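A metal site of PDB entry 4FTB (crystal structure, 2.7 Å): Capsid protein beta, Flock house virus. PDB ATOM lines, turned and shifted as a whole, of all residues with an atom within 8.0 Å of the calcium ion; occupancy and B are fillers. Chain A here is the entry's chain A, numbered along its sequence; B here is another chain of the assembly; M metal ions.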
ATOM      1  N   THR A 216      24.605  15.657  -6.329  1.00  0.00           N
ATOM      2  CA  THR A 216      23.803  14.916  -5.383  1.00  0.00           C
ATOM      3  C   THR A 216      24.471  15.034  -4.021  1.00  0.00           C
ATOM      4  O   THR A 216      25.678  14.859  -3.904  1.00  0.00           O
ATOM      5  CB  THR A 216      23.649  13.424  -5.778  1.00  0.00           C
ATOM      6  OG1 THR A 216      22.801  12.773  -4.818  1.00  0.00           O
ATOM      7  CG2 THR A 216      24.992  12.717  -5.805  1.00  0.00           C
ATOM      8  N   LEU A 217      23.693  15.379  -3.011  1.00  0.00           N
ATOM      9  CA  LEU A 217      24.219  15.517  -1.670  1.00  0.00           C
ATOM     10  C   LEU A 217      24.322  14.171  -0.954  1.00  0.00           C
ATOM     11  O   LEU A 217      23.311  13.462  -0.792  1.00  0.00           O
ATOM     12  CB  LEU A 217      23.360  16.472  -0.854  1.00  0.00           C
ATOM     13  CG  LEU A 217      23.389  17.948  -1.242  1.00  0.00           C
ATOM     14  CD1 LEU A 217      22.281  18.662  -0.508  1.00  0.00           C
ATOM     15  CD2 LEU A 217      24.733  18.562  -0.906  1.00  0.00           C
ATOM     16  N   VAL A 218      25.540  13.836  -0.550  1.00  0.00           N
ATOM     17  CA  VAL A 218      25.795  12.600   0.181  1.00  0.00           C
ATOM     18  C   VAL A 218      25.931  12.946   1.657  1.00  0.00           C
ATOM     19  O   VAL A 218      26.483  14.000   1.995  1.00  0.00           O
ATOM     20  CB  VAL A 218      27.088  11.917  -0.325  1.00  0.00           C
ATOM     21  CG1 VAL A 218      26.870  11.318  -1.706  1.00  0.00           C
ATOM     22  CG2 VAL A 218      28.230  12.921  -0.383  1.00  0.00           C
ATOM     23  N   GLY A 219      25.414  12.098   2.535  1.00  0.00           N
ATOM     24  CA  GLY A 219      25.522  12.360   3.957  1.00  0.00           C
ATOM     25  C   GLY A 219      24.272  12.934   4.596  1.00  0.00           C
ATOM     26  O   GLY A 219      24.241  13.133   5.821  1.00  0.00           O
ATOM     27  N   LEU A 220      23.258  13.208   3.775  1.00  0.00           N
ATOM     28  CA  LEU A 220      21.994  13.763   4.243  1.00  0.00           C
ATOM     29  C   LEU A 220      21.233  12.782   5.124  1.00  0.00           C
ATOM     30  O   LEU A 220      20.450  13.176   5.988  1.00  0.00           O
ATOM     31  CB  LEU A 220      21.121  14.148   3.062  1.00  0.00           C
ATOM     32  CG  LEU A 220      21.499  15.465   2.388  1.00  0.00           C
ATOM     33  CD1 LEU A 220      20.663  15.692   1.153  1.00  0.00           C
ATOM     34  CD2 LEU A 220      21.289  16.582   3.371  1.00  0.00           C
ATOM     35  N   ASP A 221      21.464  11.498   4.895  1.00  0.00           N
ATOM     36  CA  ASP A 221      20.803  10.470   5.669  1.00  0.00           C
ATOM     37  C   ASP A 221      21.114  10.647   7.148  1.00  0.00           C
ATOM     38  O   ASP A 221      20.434  10.099   8.016  1.00  0.00           O
ATOM     39  CB  ASP A 221      21.229   9.078   5.171  1.00  0.00           C
ATOM     40  CG  ASP A 221      20.644   8.740   3.778  1.00  0.00           C
ATOM     41  OD1 ASP A 221      19.420   8.550   3.654  1.00  0.00           O
ATOM     42  OD2 ASP A 221      21.438   8.676   2.798  1.00  0.00           O
ATOM     43  N   LEU A 224      18.296  11.994   9.437  1.00  0.00           N
ATOM     44  CA  LEU A 224      17.143  11.183   9.770  1.00  0.00           C
ATOM     45  C   LEU A 224      17.217  10.485  11.114  1.00  0.00           C
ATOM     46  O   LEU A 224      16.467   9.543  11.379  1.00  0.00           O
ATOM     47  CB  LEU A 224      16.890  10.168   8.656  1.00  0.00           C
ATOM     48  CG  LEU A 224      16.817  10.777   7.256  1.00  0.00           C
ATOM     49  CD1 LEU A 224      16.367   9.713   6.296  1.00  0.00           C
ATOM     50  CD2 LEU A 224      15.868  11.949   7.195  1.00  0.00           C
ATOM     51  N   LEU A 269      14.006  12.081  -7.147  1.00  0.00           N
ATOM     52  CA  LEU A 269      14.722  11.899  -5.905  1.00  0.00           C
ATOM     53  C   LEU A 269      15.278  10.471  -5.836  1.00  0.00           C
ATOM     54  O   LEU A 269      16.307  10.216  -5.221  1.00  0.00           O
ATOM     55  CB  LEU A 269      13.781  12.146  -4.717  1.00  0.00           C
ATOM     56  CG  LEU A 269      14.400  12.191  -3.322  1.00  0.00           C
ATOM     57  CD1 LEU A 269      15.398  13.340  -3.244  1.00  0.00           C
ATOM     58  CD2 LEU A 269      13.322  12.371  -2.274  1.00  0.00           C
ATOM     59  N   THR A 272      18.827  10.159  -7.342  1.00  0.00           N
ATOM     60  CA  THR A 272      19.921  10.741  -6.565  1.00  0.00           C
ATOM     61  C   THR A 272      20.384  10.028  -5.301  1.00  0.00           C
ATOM     62  O   THR A 272      21.542  10.146  -4.917  1.00  0.00           O
ATOM     63  CB  THR A 272      19.581  12.192  -6.173  1.00  0.00           C
ATOM     64  OG1 THR A 272      18.510  12.182  -5.215  1.00  0.00           O
ATOM     65  CG2 THR A 272      19.151  12.989  -7.391  1.00  0.00           C
ATOM     66  N   GLY A 273      19.501   9.288  -4.657  1.00  0.00           N
ATOM     67  CA  GLY A 273      19.902   8.630  -3.430  1.00  0.00           C
ATOM     68  C   GLY A 273      19.761   9.570  -2.240  1.00  0.00           C
ATOM     69  O   GLY A 273      20.107   9.206  -1.128  1.00  0.00           O
ATOM     70  N   GLN A 274      19.276  10.787  -2.459  1.00  0.00           N
ATOM     71  CA  GLN A 274      19.106  11.716  -1.347  1.00  0.00           C
ATOM     72  C   GLN A 274      17.847  11.335  -0.602  1.00  0.00           C
ATOM     73  O   GLN A 274      16.872  10.894  -1.197  1.00  0.00           O
ATOM     74  CB  GLN A 274      18.960  13.142  -1.844  1.00  0.00           C
ATOM     75  CG  GLN A 274      20.174  13.684  -2.570  1.00  0.00           C
ATOM     76  CD  GLN A 274      20.027  15.162  -2.872  1.00  0.00           C
ATOM     77  OE1 GLN A 274      20.812  15.732  -3.622  1.00  0.00           O
ATOM     78  NE2 GLN A 274      19.010  15.793  -2.289  1.00  0.00           N
ATOM     79  N   PRO A 275      17.831  11.505   0.735  1.00  0.00           N
ATOM     80  CA  PRO A 275      16.640  11.170   1.523  1.00  0.00           C
ATOM     81  C   PRO A 275      15.523  12.206   1.397  1.00  0.00           C
ATOM     82  O   PRO A 275      14.361  11.919   1.719  1.00  0.00           O
ATOM     83  CB  PRO A 275      17.202  11.072   2.940  1.00  0.00           C
ATOM     84  CG  PRO A 275      18.267  12.109   2.930  1.00  0.00           C
ATOM     85  CD  PRO A 275      18.955  11.861   1.610  1.00  0.00           C
ATOM     86  N   PHE A 276      15.854  13.409   0.938  1.00  0.00           N
ATOM     87  CA  PHE A 276      14.852  14.453   0.780  1.00  0.00           C
ATOM     88  C   PHE A 276      15.327  15.539  -0.181  1.00  0.00           C
ATOM     89  O   PHE A 276      16.390  15.421  -0.792  1.00  0.00           O
ATOM     90  CB  PHE A 276      14.461  15.048   2.129  1.00  0.00           C
ATOM     91  CG  PHE A 276      15.621  15.479   2.972  1.00  0.00           C
ATOM     92  CD1 PHE A 276      16.321  16.648   2.673  1.00  0.00           C
ATOM     93  CD2 PHE A 276      16.020  14.706   4.065  1.00  0.00           C
ATOM     94  CE1 PHE A 276      17.418  17.035   3.452  1.00  0.00           C
ATOM     95  CE2 PHE A 276      17.115  15.083   4.844  1.00  0.00           C
ATOM     96  CZ  PHE A 276      17.814  16.253   4.530  1.00  0.00           C
ATOM     97  N   THR B 155      22.080  -1.191  -3.592  1.00  0.00           N
ATOM     98  CA  THR B 155      21.595  -0.557  -4.810  1.00  0.00           C
ATOM     99  C   THR B 155      22.622   0.514  -5.128  1.00  0.00           C
ATOM    100  O   THR B 155      23.233   1.077  -4.226  1.00  0.00           O
ATOM    101  CB  THR B 155      20.215   0.097  -4.607  1.00  0.00           C
ATOM    102  OG1 THR B 155      20.376   1.430  -4.130  1.00  0.00           O
ATOM    103  CG2 THR B 155      19.398  -0.695  -3.600  1.00  0.00           C
ATOM    104  N   THR B 157      22.450   3.425  -5.563  1.00  0.00           N
ATOM    105  CA  THR B 157      22.181   4.751  -5.012  1.00  0.00           C
ATOM    106  C   THR B 157      22.061   4.789  -3.480  1.00  0.00           C
ATOM    107  O   THR B 157      21.449   5.705  -2.896  1.00  0.00           O
ATOM    108  CB  THR B 157      20.924   5.383  -5.652  1.00  0.00           C
ATOM    109  OG1 THR B 157      19.815   4.481  -5.511  1.00  0.00           O
ATOM    110  CG2 THR B 157      21.180   5.641  -7.129  1.00  0.00           C
ATOM    111  N   SER B 158      22.660   3.804  -2.841  1.00  0.00           N
ATOM    112  CA  SER B 158      22.653   3.741  -1.384  1.00  0.00           C
ATOM    113  C   SER B 158      24.092   3.609  -0.863  1.00  0.00           C
ATOM    114  O   SER B 158      24.334   3.094   0.231  1.00  0.00           O
ATOM    115  CB  SER B 158      21.770   2.560  -0.922  1.00  0.00           C
ATOM    116  OG  SER B 158      22.039   1.387  -1.670  1.00  0.00           O
ATOM    117  N   ARG B 159      25.034   4.109  -1.652  1.00  0.00           N
ATOM    118  CA  ARG B 159      26.449   4.042  -1.296  1.00  0.00           C
ATOM    119  C   ARG B 159      26.836   5.009  -0.190  1.00  0.00           C
ATOM    120  O   ARG B 159      27.753   4.728   0.584  1.00  0.00           O
ATOM    121  CB  ARG B 159      27.311   4.305  -2.528  1.00  0.00           C
ATOM    122  CG  ARG B 159      26.971   3.456  -3.742  1.00  0.00           C
ATOM    123  CD  ARG B 159      26.800   2.000  -3.376  1.00  0.00           C
ATOM    124  NE  ARG B 159      26.723   1.156  -4.557  1.00  0.00           N
ATOM    125  CZ  ARG B 159      26.373  -0.131  -4.549  1.00  0.00           C
ATOM    126  NH1 ARG B 159      26.068  -0.721  -3.395  1.00  0.00           N
ATOM    127  NH2 ARG B 159      26.351  -0.826  -5.675  1.00  0.00           N
ATOM    128  N   SER B 160      26.141   6.141  -0.101  1.00  0.00           N
ATOM    129  CA  SER B 160      26.446   7.149   0.926  1.00  0.00           C
ATOM    130  C   SER B 160      25.535   7.041   2.148  1.00  0.00           C
ATOM    131  O   SER B 160      25.375   8.007   2.886  1.00  0.00           O
ATOM    132  CB  SER B 160      26.317   8.547   0.327  1.00  0.00           C
ATOM    133  OG  SER B 160      24.952   8.864   0.077  1.00  0.00           O
ATOM    134  N   ASP B 161      24.946   5.873   2.372  1.00  0.00           N
ATOM    135  CA  ASP B 161      24.032   5.740   3.486  1.00  0.00           C
ATOM    136  C   ASP B 161      24.696   5.624   4.848  1.00  0.00           C
ATOM    137  O   ASP B 161      24.204   6.177   5.831  1.00  0.00           O
ATOM    138  CB  ASP B 161      23.102   4.544   3.247  1.00  0.00           C
ATOM    139  CG  ASP B 161      22.018   4.854   2.197  1.00  0.00           C
ATOM    140  OD1 ASP B 161      22.326   5.497   1.174  1.00  0.00           O
ATOM    141  OD2 ASP B 161      20.864   4.430   2.383  1.00  0.00           O
ATOM    142  N   GLN B 162      25.827   4.926   4.901  1.00  0.00           N
ATOM    143  CA  GLN B 162      26.561   4.761   6.144  1.00  0.00           C
ATOM    144  C   GLN B 162      27.650   5.823   6.341  1.00  0.00           C
ATOM    145  O   GLN B 162      27.796   6.391   7.432  1.00  0.00           O
ATOM    146  CB  GLN B 162      27.206   3.376   6.205  1.00  0.00           C
ATOM    147  CG  GLN B 162      26.233   2.225   6.070  1.00  0.00           C
ATOM    148  CD  GLN B 162      25.017   2.370   6.972  1.00  0.00           C
ATOM    149  OE1 GLN B 162      25.146   2.536   8.196  1.00  0.00           O
ATOM    150  NE2 GLN B 162      23.843   2.296   6.378  1.00  0.00           N
ATOM    151  N   GLU B 257      27.960   8.173  -6.009  1.00  0.00           N
ATOM    152  CA  GLU B 257      26.694   7.462  -6.142  1.00  0.00           C
ATOM    153  C   GLU B 257      26.266   7.081  -7.550  1.00  0.00           C
ATOM    154  O   GLU B 257      26.365   7.875  -8.471  1.00  0.00           O
ATOM    155  CB  GLU B 257      25.577   8.295  -5.499  1.00  0.00           C
ATOM    156  CG  GLU B 257      25.636   8.399  -3.992  1.00  0.00           C
ATOM    157  CD  GLU B 257      25.083   7.179  -3.298  1.00  0.00           C
ATOM    158  OE1 GLU B 257      24.831   7.251  -2.078  1.00  0.00           O
ATOM    159  OE2 GLU B 257      24.901   6.147  -3.970  1.00  0.00           O
ATOM    160  N   ASN B 324      28.130   8.752   9.098  1.00  0.00           N
ATOM    161  CA  ASN B 324      26.871   9.471   9.144  1.00  0.00           C
ATOM    162  C   ASN B 324      26.259   9.231  10.516  1.00  0.00           C
ATOM    163  O   ASN B 324      26.156   8.084  10.955  1.00  0.00           O
ATOM    164  CB  ASN B 324      25.936   8.964   8.068  1.00  0.00           C
ATOM    165  CG  ASN B 324      26.303   9.489   6.708  1.00  0.00           C
ATOM    166  OD1 ASN B 324      26.162   8.783   5.708  1.00  0.00           O
ATOM    167  ND2 ASN B 324      26.752  10.738   6.659  1.00  0.00           N
HETATM  168 CA    CA M   1      20.930   7.595   0.415  1.00  0.00          CA
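O of Thr 157 of chain B touches the calcium ion, at 3.8 Å. Within 4 Å of the calcium ion: Asp 221, Gly 273, Thr 157 of chain B and Asp 161 of chain B. The nearest printed residue that does not touch the calcium ion is Ser 160 of chain B (4.2 Å).
The calcium ion is bound by O of Gly 273. The calcium ion is bound by the side-chain carboxylate (OD1) of Asp 161 of chain B (2.6 Å). OD2 of Asp 221 is bound to the calcium ion, at 2.7 Å. The calcium ion has three donor atoms within binding distance.
The backbone carbonyl oxygen (O) of Asp 161 of chain B sits close to the side-chain amide oxygen (OD1) of Asn 324 of chain B (3.3 Å). OG1 of Thr 155 of chain B sits close to N of Thr 157 of chain B, at 3.2 Å.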
